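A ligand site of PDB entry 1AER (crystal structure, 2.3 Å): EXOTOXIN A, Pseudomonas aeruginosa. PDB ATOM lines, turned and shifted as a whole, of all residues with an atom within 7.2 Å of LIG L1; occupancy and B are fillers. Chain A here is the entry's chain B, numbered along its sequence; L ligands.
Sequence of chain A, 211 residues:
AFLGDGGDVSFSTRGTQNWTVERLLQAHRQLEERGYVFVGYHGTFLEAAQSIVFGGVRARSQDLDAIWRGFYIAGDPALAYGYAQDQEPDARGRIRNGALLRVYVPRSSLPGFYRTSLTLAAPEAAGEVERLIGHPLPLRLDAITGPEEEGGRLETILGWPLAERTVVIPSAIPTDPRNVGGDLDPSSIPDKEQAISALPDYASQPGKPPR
The side-chain carboxylate (OE1) of Glu 155 sits close to a sulfur (S1) of LIG L1, 2.9 Å away. His 42 touches LIG L1. Tyr 72 touches LIG L1 (CB to C1, 3.4 Å). Ala 80 touches LIG L1. Hydrophobic or aromatic side chains within 4 Å of LIG L1: His 42, Tyr 72, Ala 80 and Tyr 83. Within 4 Å of LIG L1: His 42, Gly 43, Tyr 72, Ala 80, Tyr 83 and Glu 155.
A ring nitrogen (ND1) of His 42 lies within hydrogen-bond range of the backbone carbonyl oxygen (O) of Tyr 72, 2.6 Å away.
The backbone NH (N) of Gly 43 lies within hydrogen-bond range of an oxygen (O1) of LIG L1 (2.7 Å). The backbone carbonyl oxygen (O) of Gly 43 is in hydrogen-bond range of a nitrogen (N2) of LIG L1, 2.8 Å away. OH of Tyr 83 sits close to S1 of LIG L1. A ring nitrogen (NE2) of His 42 lies within hydrogen-bond range of an oxygen (O6) of LG2 L2. The side-chain hydroxyl (OG1) of Thr 44 lies within hydrogen-bond range of an oxygen (O6) of LG2 L2 (2.8 Å).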
ATOM      1  N   TYR A  41     -25.994 -15.964 -20.849  1.00  0.00           N
ATOM      2  CA  TYR A  41     -25.574 -15.500 -19.538  1.00  0.00           C
ATOM      3  C   TYR A  41     -24.519 -16.410 -18.899  1.00  0.00           C
ATOM      4  O   TYR A  41     -24.431 -17.607 -19.176  1.00  0.00           O
ATOM      5  CB  TYR A  41     -26.782 -15.482 -18.607  1.00  0.00           C
ATOM      6  CG  TYR A  41     -27.849 -14.526 -19.012  1.00  0.00           C
ATOM      7  CD1 TYR A  41     -28.827 -14.889 -19.927  1.00  0.00           C
ATOM      8  CD2 TYR A  41     -27.896 -13.250 -18.461  1.00  0.00           C
ATOM      9  CE1 TYR A  41     -29.850 -13.982 -20.276  1.00  0.00           C
ATOM     10  CE2 TYR A  41     -28.907 -12.348 -18.814  1.00  0.00           C
ATOM     11  CZ  TYR A  41     -29.877 -12.727 -19.705  1.00  0.00           C
ATOM     12  OH  TYR A  41     -30.900 -11.835 -20.010  1.00  0.00           O
ATOM     13  N   HIS A  42     -23.715 -15.799 -18.054  1.00  0.00           N
ATOM     14  CA  HIS A  42     -22.725 -16.542 -17.291  1.00  0.00           C
ATOM     15  C   HIS A  42     -22.949 -16.146 -15.813  1.00  0.00           C
ATOM     16  O   HIS A  42     -22.878 -14.980 -15.506  1.00  0.00           O
ATOM     17  CB  HIS A  42     -21.314 -16.125 -17.699  1.00  0.00           C
ATOM     18  CG  HIS A  42     -20.242 -16.891 -16.977  1.00  0.00           C
ATOM     19  ND1 HIS A  42     -20.003 -18.228 -17.241  1.00  0.00           N
ATOM     20  CD2 HIS A  42     -19.425 -16.555 -15.963  1.00  0.00           C
ATOM     21  CE1 HIS A  42     -19.093 -18.683 -16.403  1.00  0.00           C
ATOM     22  NE2 HIS A  42     -18.716 -17.682 -15.611  1.00  0.00           N
ATOM     23  N   GLY A  43     -23.310 -17.077 -14.914  1.00  0.00           N
ATOM     24  CA  GLY A  43     -23.479 -16.700 -13.513  1.00  0.00           C
ATOM     25  C   GLY A  43     -22.212 -17.057 -12.715  1.00  0.00           C
ATOM     26  O   GLY A  43     -21.707 -18.172 -12.880  1.00  0.00           O
ATOM     27  N   THR A  44     -21.673 -16.160 -11.900  1.00  0.00           N
ATOM     28  CA  THR A  44     -20.475 -16.524 -11.172  1.00  0.00           C
ATOM     29  C   THR A  44     -20.343 -15.709  -9.865  1.00  0.00           C
ATOM     30  O   THR A  44     -21.256 -14.957  -9.543  1.00  0.00           O
ATOM     31  CB  THR A  44     -19.258 -16.369 -12.063  1.00  0.00           C
ATOM     32  OG1 THR A  44     -18.086 -16.889 -11.404  1.00  0.00           O
ATOM     33  CG2 THR A  44     -19.044 -14.921 -12.401  1.00  0.00           C
ATOM     34  N   GLY A  70     -13.967 -25.334 -21.866  1.00  0.00           N
ATOM     35  CA  GLY A  70     -14.575 -24.204 -22.531  1.00  0.00           C
ATOM     36  C   GLY A  70     -15.170 -23.313 -21.456  1.00  0.00           C
ATOM     37  O   GLY A  70     -15.013 -23.576 -20.274  1.00  0.00           O
ATOM     38  N   PHE A  71     -15.809 -22.215 -21.873  1.00  0.00           N
ATOM     39  CA  PHE A  71     -16.470 -21.244 -20.988  1.00  0.00           C
ATOM     40  C   PHE A  71     -17.949 -21.490 -21.122  1.00  0.00           C
ATOM     41  O   PHE A  71     -18.514 -21.337 -22.228  1.00  0.00           O
ATOM     42  CB  PHE A  71     -16.176 -19.823 -21.485  1.00  0.00           C
ATOM     43  CG  PHE A  71     -16.562 -18.740 -20.510  1.00  0.00           C
ATOM     44  CD1 PHE A  71     -15.892 -18.608 -19.293  1.00  0.00           C
ATOM     45  CD2 PHE A  71     -17.494 -17.777 -20.867  1.00  0.00           C
ATOM     46  CE1 PHE A  71     -16.128 -17.530 -18.475  1.00  0.00           C
ATOM     47  CE2 PHE A  71     -17.747 -16.695 -20.057  1.00  0.00           C
ATOM     48  CZ  PHE A  71     -17.063 -16.575 -18.853  1.00  0.00           C
ATOM     49  N   TYR A  72     -18.569 -21.848 -20.001  1.00  0.00           N
ATOM     50  CA  TYR A  72     -20.011 -22.151 -19.944  1.00  0.00           C
ATOM     51  C   TYR A  72     -20.955 -20.974 -19.750  1.00  0.00           C
ATOM     52  O   TYR A  72     -20.769 -20.114 -18.856  1.00  0.00           O
ATOM     53  CB  TYR A  72     -20.302 -23.208 -18.853  1.00  0.00           C
ATOM     54  CG  TYR A  72     -19.836 -24.613 -19.198  1.00  0.00           C
ATOM     55  CD1 TYR A  72     -18.471 -24.934 -19.177  1.00  0.00           C
ATOM     56  CD2 TYR A  72     -20.755 -25.614 -19.495  1.00  0.00           C
ATOM     57  CE1 TYR A  72     -18.038 -26.219 -19.456  1.00  0.00           C
ATOM     58  CE2 TYR A  72     -20.332 -26.925 -19.763  1.00  0.00           C
ATOM     59  CZ  TYR A  72     -18.972 -27.210 -19.741  1.00  0.00           C
ATOM     60  OH  TYR A  72     -18.528 -28.474 -20.040  1.00  0.00           O
ATOM     61  N   ILE A  73     -21.965 -20.926 -20.581  1.00  0.00           N
ATOM     62  CA  ILE A  73     -22.945 -19.869 -20.514  1.00  0.00           C
ATOM     63  C   ILE A  73     -24.271 -20.559 -20.789  1.00  0.00           C
ATOM     64  O   ILE A  73     -24.307 -21.734 -21.199  1.00  0.00           O
ATOM     65  CB  ILE A  73     -22.685 -18.778 -21.576  1.00  0.00           C
ATOM     66  CG1 ILE A  73     -22.881 -19.332 -22.969  1.00  0.00           C
ATOM     67  CG2 ILE A  73     -21.288 -18.277 -21.446  1.00  0.00           C
ATOM     68  CD1 ILE A  73     -22.692 -18.311 -24.067  1.00  0.00           C
ATOM     69  N   ALA A  74     -25.363 -19.847 -20.550  1.00  0.00           N
ATOM     70  CA  ALA A  74     -26.695 -20.405 -20.816  1.00  0.00           C
ATOM     71  C   ALA A  74     -27.628 -19.349 -21.333  1.00  0.00           C
ATOM     72  O   ALA A  74     -27.626 -18.218 -20.841  1.00  0.00           O
ATOM     73  CB  ALA A  74     -27.266 -21.015 -19.549  1.00  0.00           C
ATOM     74  N   LEU A  79     -31.081 -20.698 -15.566  1.00  0.00           N
ATOM     75  CA  LEU A  79     -30.028 -21.698 -15.576  1.00  0.00           C
ATOM     76  C   LEU A  79     -28.759 -21.086 -14.990  1.00  0.00           C
ATOM     77  O   LEU A  79     -28.274 -21.550 -13.958  1.00  0.00           O
ATOM     78  CB  LEU A  79     -29.784 -22.226 -16.998  1.00  0.00           C
ATOM     79  CG  LEU A  79     -28.666 -23.232 -17.317  1.00  0.00           C
ATOM     80  CD1 LEU A  79     -28.082 -23.830 -16.089  1.00  0.00           C
ATOM     81  CD2 LEU A  79     -29.195 -24.315 -18.241  1.00  0.00           C
ATOM     82  N   ALA A  80     -28.269 -20.003 -15.611  1.00  0.00           N
ATOM     83  CA  ALA A  80     -27.049 -19.343 -15.142  1.00  0.00           C
ATOM     84  C   ALA A  80     -27.158 -18.875 -13.696  1.00  0.00           C
ATOM     85  O   ALA A  80     -26.172 -18.882 -12.946  1.00  0.00           O
ATOM     86  CB  ALA A  80     -26.707 -18.179 -16.020  1.00  0.00           C
ATOM     87  N   TYR A  81     -28.379 -18.477 -13.307  1.00  0.00           N
ATOM     88  CA  TYR A  81     -28.653 -18.006 -11.961  1.00  0.00           C
ATOM     89  C   TYR A  81     -28.213 -19.113 -10.975  1.00  0.00           C
ATOM     90  O   TYR A  81     -27.944 -18.854  -9.789  1.00  0.00           O
ATOM     91  CB  TYR A  81     -30.148 -17.730 -11.765  1.00  0.00           C
ATOM     92  CG  TYR A  81     -30.457 -17.008 -10.476  1.00  0.00           C
ATOM     93  CD1 TYR A  81     -30.233 -15.634 -10.359  1.00  0.00           C
ATOM     94  CD2 TYR A  81     -30.942 -17.710  -9.353  1.00  0.00           C
ATOM     95  CE1 TYR A  81     -30.459 -14.960  -9.168  1.00  0.00           C
ATOM     96  CE2 TYR A  81     -31.171 -17.032  -8.130  1.00  0.00           C
ATOM     97  CZ  TYR A  81     -30.928 -15.659  -8.053  1.00  0.00           C
ATOM     98  OH  TYR A  81     -31.156 -14.952  -6.894  1.00  0.00           O
ATOM     99  N   GLY A  82     -28.160 -20.346 -11.475  1.00  0.00           N
ATOM    100  CA  GLY A  82     -27.750 -21.473 -10.670  1.00  0.00           C
ATOM    101  C   GLY A  82     -26.378 -21.286 -10.062  1.00  0.00           C
ATOM    102  O   GLY A  82     -26.031 -21.982  -9.099  1.00  0.00           O
ATOM    103  N   TYR A  83     -25.601 -20.340 -10.607  1.00  0.00           N
ATOM    104  CA  TYR A  83     -24.254 -20.063 -10.131  1.00  0.00           C
ATOM    105  C   TYR A  83     -23.933 -18.694  -9.432  1.00  0.00           C
ATOM    106  O   TYR A  83     -24.465 -17.589  -9.741  1.00  0.00           O
ATOM    107  CB  TYR A  83     -23.258 -20.445 -11.205  1.00  0.00           C
ATOM    108  CG  TYR A  83     -23.615 -21.740 -11.921  1.00  0.00           C
ATOM    109  CD1 TYR A  83     -24.657 -21.769 -12.854  1.00  0.00           C
ATOM    110  CD2 TYR A  83     -22.920 -22.920 -11.678  1.00  0.00           C
ATOM    111  CE1 TYR A  83     -24.987 -22.935 -13.536  1.00  0.00           C
ATOM    112  CE2 TYR A  83     -23.241 -24.100 -12.361  1.00  0.00           C
ATOM    113  CZ  TYR A  83     -24.292 -24.100 -13.288  1.00  0.00           C
ATOM    114  OH  TYR A  83     -24.650 -25.263 -13.959  1.00  0.00           O
ATOM    115  N   ALA A  84     -23.172 -18.883  -8.329  1.00  0.00           N
ATOM    116  CA  ALA A  84     -22.691 -17.843  -7.387  1.00  0.00           C
ATOM    117  C   ALA A  84     -21.516 -18.421  -6.537  1.00  0.00           C
ATOM    118  O   ALA A  84     -20.731 -19.253  -7.019  1.00  0.00           O
ATOM    119  CB  ALA A  84     -23.838 -17.380  -6.488  1.00  0.00           C
ATOM    120  N   ALA A  99     -22.776 -12.869  -9.266  1.00  0.00           N
ATOM    121  CA  ALA A  99     -23.279 -12.009 -10.320  1.00  0.00           C
ATOM    122  C   ALA A  99     -23.570 -12.684 -11.645  1.00  0.00           C
ATOM    123  O   ALA A  99     -22.967 -13.699 -12.010  1.00  0.00           O
ATOM    124  CB  ALA A  99     -22.356 -10.820 -10.522  1.00  0.00           C
ATOM    125  N   LEU A 100     -24.582 -12.155 -12.286  1.00  0.00           N
ATOM    126  CA  LEU A 100     -24.982 -12.612 -13.592  1.00  0.00           C
ATOM    127  C   LEU A 100     -24.372 -11.634 -14.604  1.00  0.00           C
ATOM    128  O   LEU A 100     -24.420 -10.416 -14.407  1.00  0.00           O
ATOM    129  CB  LEU A 100     -26.503 -12.655 -13.686  1.00  0.00           C
ATOM    130  CG  LEU A 100     -27.114 -13.966 -13.165  1.00  0.00           C
ATOM    131  CD1 LEU A 100     -28.520 -13.715 -12.740  1.00  0.00           C
ATOM    132  CD2 LEU A 100     -27.084 -15.035 -14.211  1.00  0.00           C
ATOM    133  N   ALA A 121     -20.511 -33.043 -22.157  1.00  0.00           N
ATOM    134  CA  ALA A 121     -19.534 -33.508 -21.179  1.00  0.00           C
ATOM    135  C   ALA A 121     -19.837 -34.888 -20.648  1.00  0.00           C
ATOM    136  O   ALA A 121     -19.565 -35.229 -19.500  1.00  0.00           O
ATOM    137  CB  ALA A 121     -19.382 -32.499 -20.043  1.00  0.00           C
ATOM    138  N   GLU A 155     -27.519 -25.665 -22.230  1.00  0.00           N
ATOM    139  CA  GLU A 155     -26.351 -24.899 -21.877  1.00  0.00           C
ATOM    140  C   GLU A 155     -25.387 -24.882 -23.063  1.00  0.00           C
ATOM    141  O   GLU A 155     -25.488 -25.718 -23.963  1.00  0.00           O
ATOM    142  CB  GLU A 155     -25.720 -25.336 -20.528  1.00  0.00           C
ATOM    143  CG  GLU A 155     -25.217 -26.767 -20.362  1.00  0.00           C
ATOM    144  CD  GLU A 155     -24.459 -26.950 -19.034  1.00  0.00           C
ATOM    145  OE1 GLU A 155     -24.751 -26.195 -18.058  1.00  0.00           O
ATOM    146  OE2 GLU A 155     -23.553 -27.826 -18.951  1.00  0.00           O
ATOM    147  N   THR A 156     -24.554 -23.842 -23.097  1.00  0.00           N
ATOM    148  CA  THR A 156     -23.570 -23.608 -24.156  1.00  0.00           C
ATOM    149  C   THR A 156     -22.137 -23.478 -23.578  1.00  0.00           C
ATOM    150  O   THR A 156     -21.927 -22.886 -22.514  1.00  0.00           O
ATOM    151  CB  THR A 156     -23.925 -22.300 -24.945  1.00  0.00           C
ATOM    152  OG1 THR A 156     -25.077 -22.521 -25.776  1.00  0.00           O
ATOM    153  CG2 THR A 156     -22.778 -21.855 -25.830  1.00  0.00           C
HETATM  154  S1  LIG L   1     -23.234 -23.913 -17.040  1.00  0.00           S
HETATM  155  C1  LIG L   1     -21.907 -23.864 -15.879  1.00  0.00           C
HETATM  156  N1  LIG L   1     -21.721 -22.641 -15.367  1.00  0.00           N
HETATM  157  C2  LIG L   1     -22.644 -21.816 -15.910  1.00  0.00           C
HETATM  158  C3  LIG L   1     -23.586 -22.197 -16.837  1.00  0.00           C
HETATM  159  C4  LIG L   1     -22.514 -20.507 -15.323  1.00  0.00           C
HETATM  160  O1  LIG L   1     -23.332 -19.650 -15.674  1.00  0.00           O
HETATM  161  N2  LIG L   1     -21.481 -20.447 -14.459  1.00  0.00           N
HETATM  162  C5  LIG L   1     -21.019 -24.928 -15.338  1.00  0.00           C
HETATM  163  C6  LIG L   1     -20.481 -26.129 -16.033  1.00  0.00           C
HETATM  164  O2  LIG L   1     -21.478 -27.216 -15.975  1.00  0.00           O
HETATM  165  C7  LIG L   1     -19.228 -26.429 -15.164  1.00  0.00           C
HETATM  166  O3  LIG L   1     -19.694 -27.242 -14.045  1.00  0.00           O
HETATM  167  C8  LIG L   1     -18.740 -25.140 -14.490  1.00  0.00           C
HETATM  168  O4  LIG L   1     -19.809 -24.241 -14.815  1.00  0.00           O
HETATM  169  C9  LIG L   1     -17.330 -24.604 -14.832  1.00  0.00           C
HETATM  170  P1  LG2 L   2     -12.494 -23.217 -15.340  1.00  0.00           P
HETATM  171  O1  LG2 L   2     -11.098 -23.210 -15.972  1.00  0.00           O
HETATM  172  O2  LG2 L   2     -13.720 -23.529 -16.257  1.00  0.00           O
HETATM  173  O3  LG2 L   2     -12.871 -21.570 -15.156  1.00  0.00           O
HETATM  174  C1  LG2 L   2     -14.268 -21.027 -15.058  1.00  0.00           C
HETATM  175  C2  LG2 L   2     -14.748 -20.658 -13.638  1.00  0.00           C
HETATM  176  O4  LG2 L   2     -13.921 -19.606 -13.054  1.00  0.00           O
HETATM  177  C3  LG2 L   2     -16.086 -19.932 -13.679  1.00  0.00           C
HETATM  178  O5  LG2 L   2     -16.676 -19.798 -12.339  1.00  0.00           O
HETATM  179  C4  LG2 L   2     -15.624 -18.532 -14.113  1.00  0.00           C
HETATM  180  O6  LG2 L   2     -16.775 -17.744 -13.770  1.00  0.00           O
HETATM  181  C5  LG2 L   2     -14.514 -18.253 -13.126  1.00  0.00           C
HETATM  182  N1  LG2 L   2     -13.573 -17.150 -13.515  1.00  0.00           N
HETATM  183  C6  LG2 L   2     -12.937 -16.302 -12.709  1.00  0.00           C
HETATM  184  N2  LG2 L   2     -12.181 -15.500 -13.423  1.00  0.00           N
HETATM  185  C7  LG2 L   2     -12.361 -15.912 -14.708  1.00  0.00           C
HETATM  186  C8  LG2 L   2     -11.860 -15.353 -15.913  1.00  0.00           C
HETATM  187  N3  LG2 L   2     -10.986 -14.331 -15.873  1.00  0.00           N
HETATM  188  N4  LG2 L   2     -12.207 -15.904 -17.100  1.00  0.00           N
HETATM  189  C9  LG2 L   2     -12.981 -16.979 -17.181  1.00  0.00           C
HETATM  190  N5  LG2 L   2     -13.514 -17.467 -16.051  1.00  0.00           N
HETATM  191  C10 LG2 L   2     -13.234 -16.946 -14.801  1.00  0.00           C
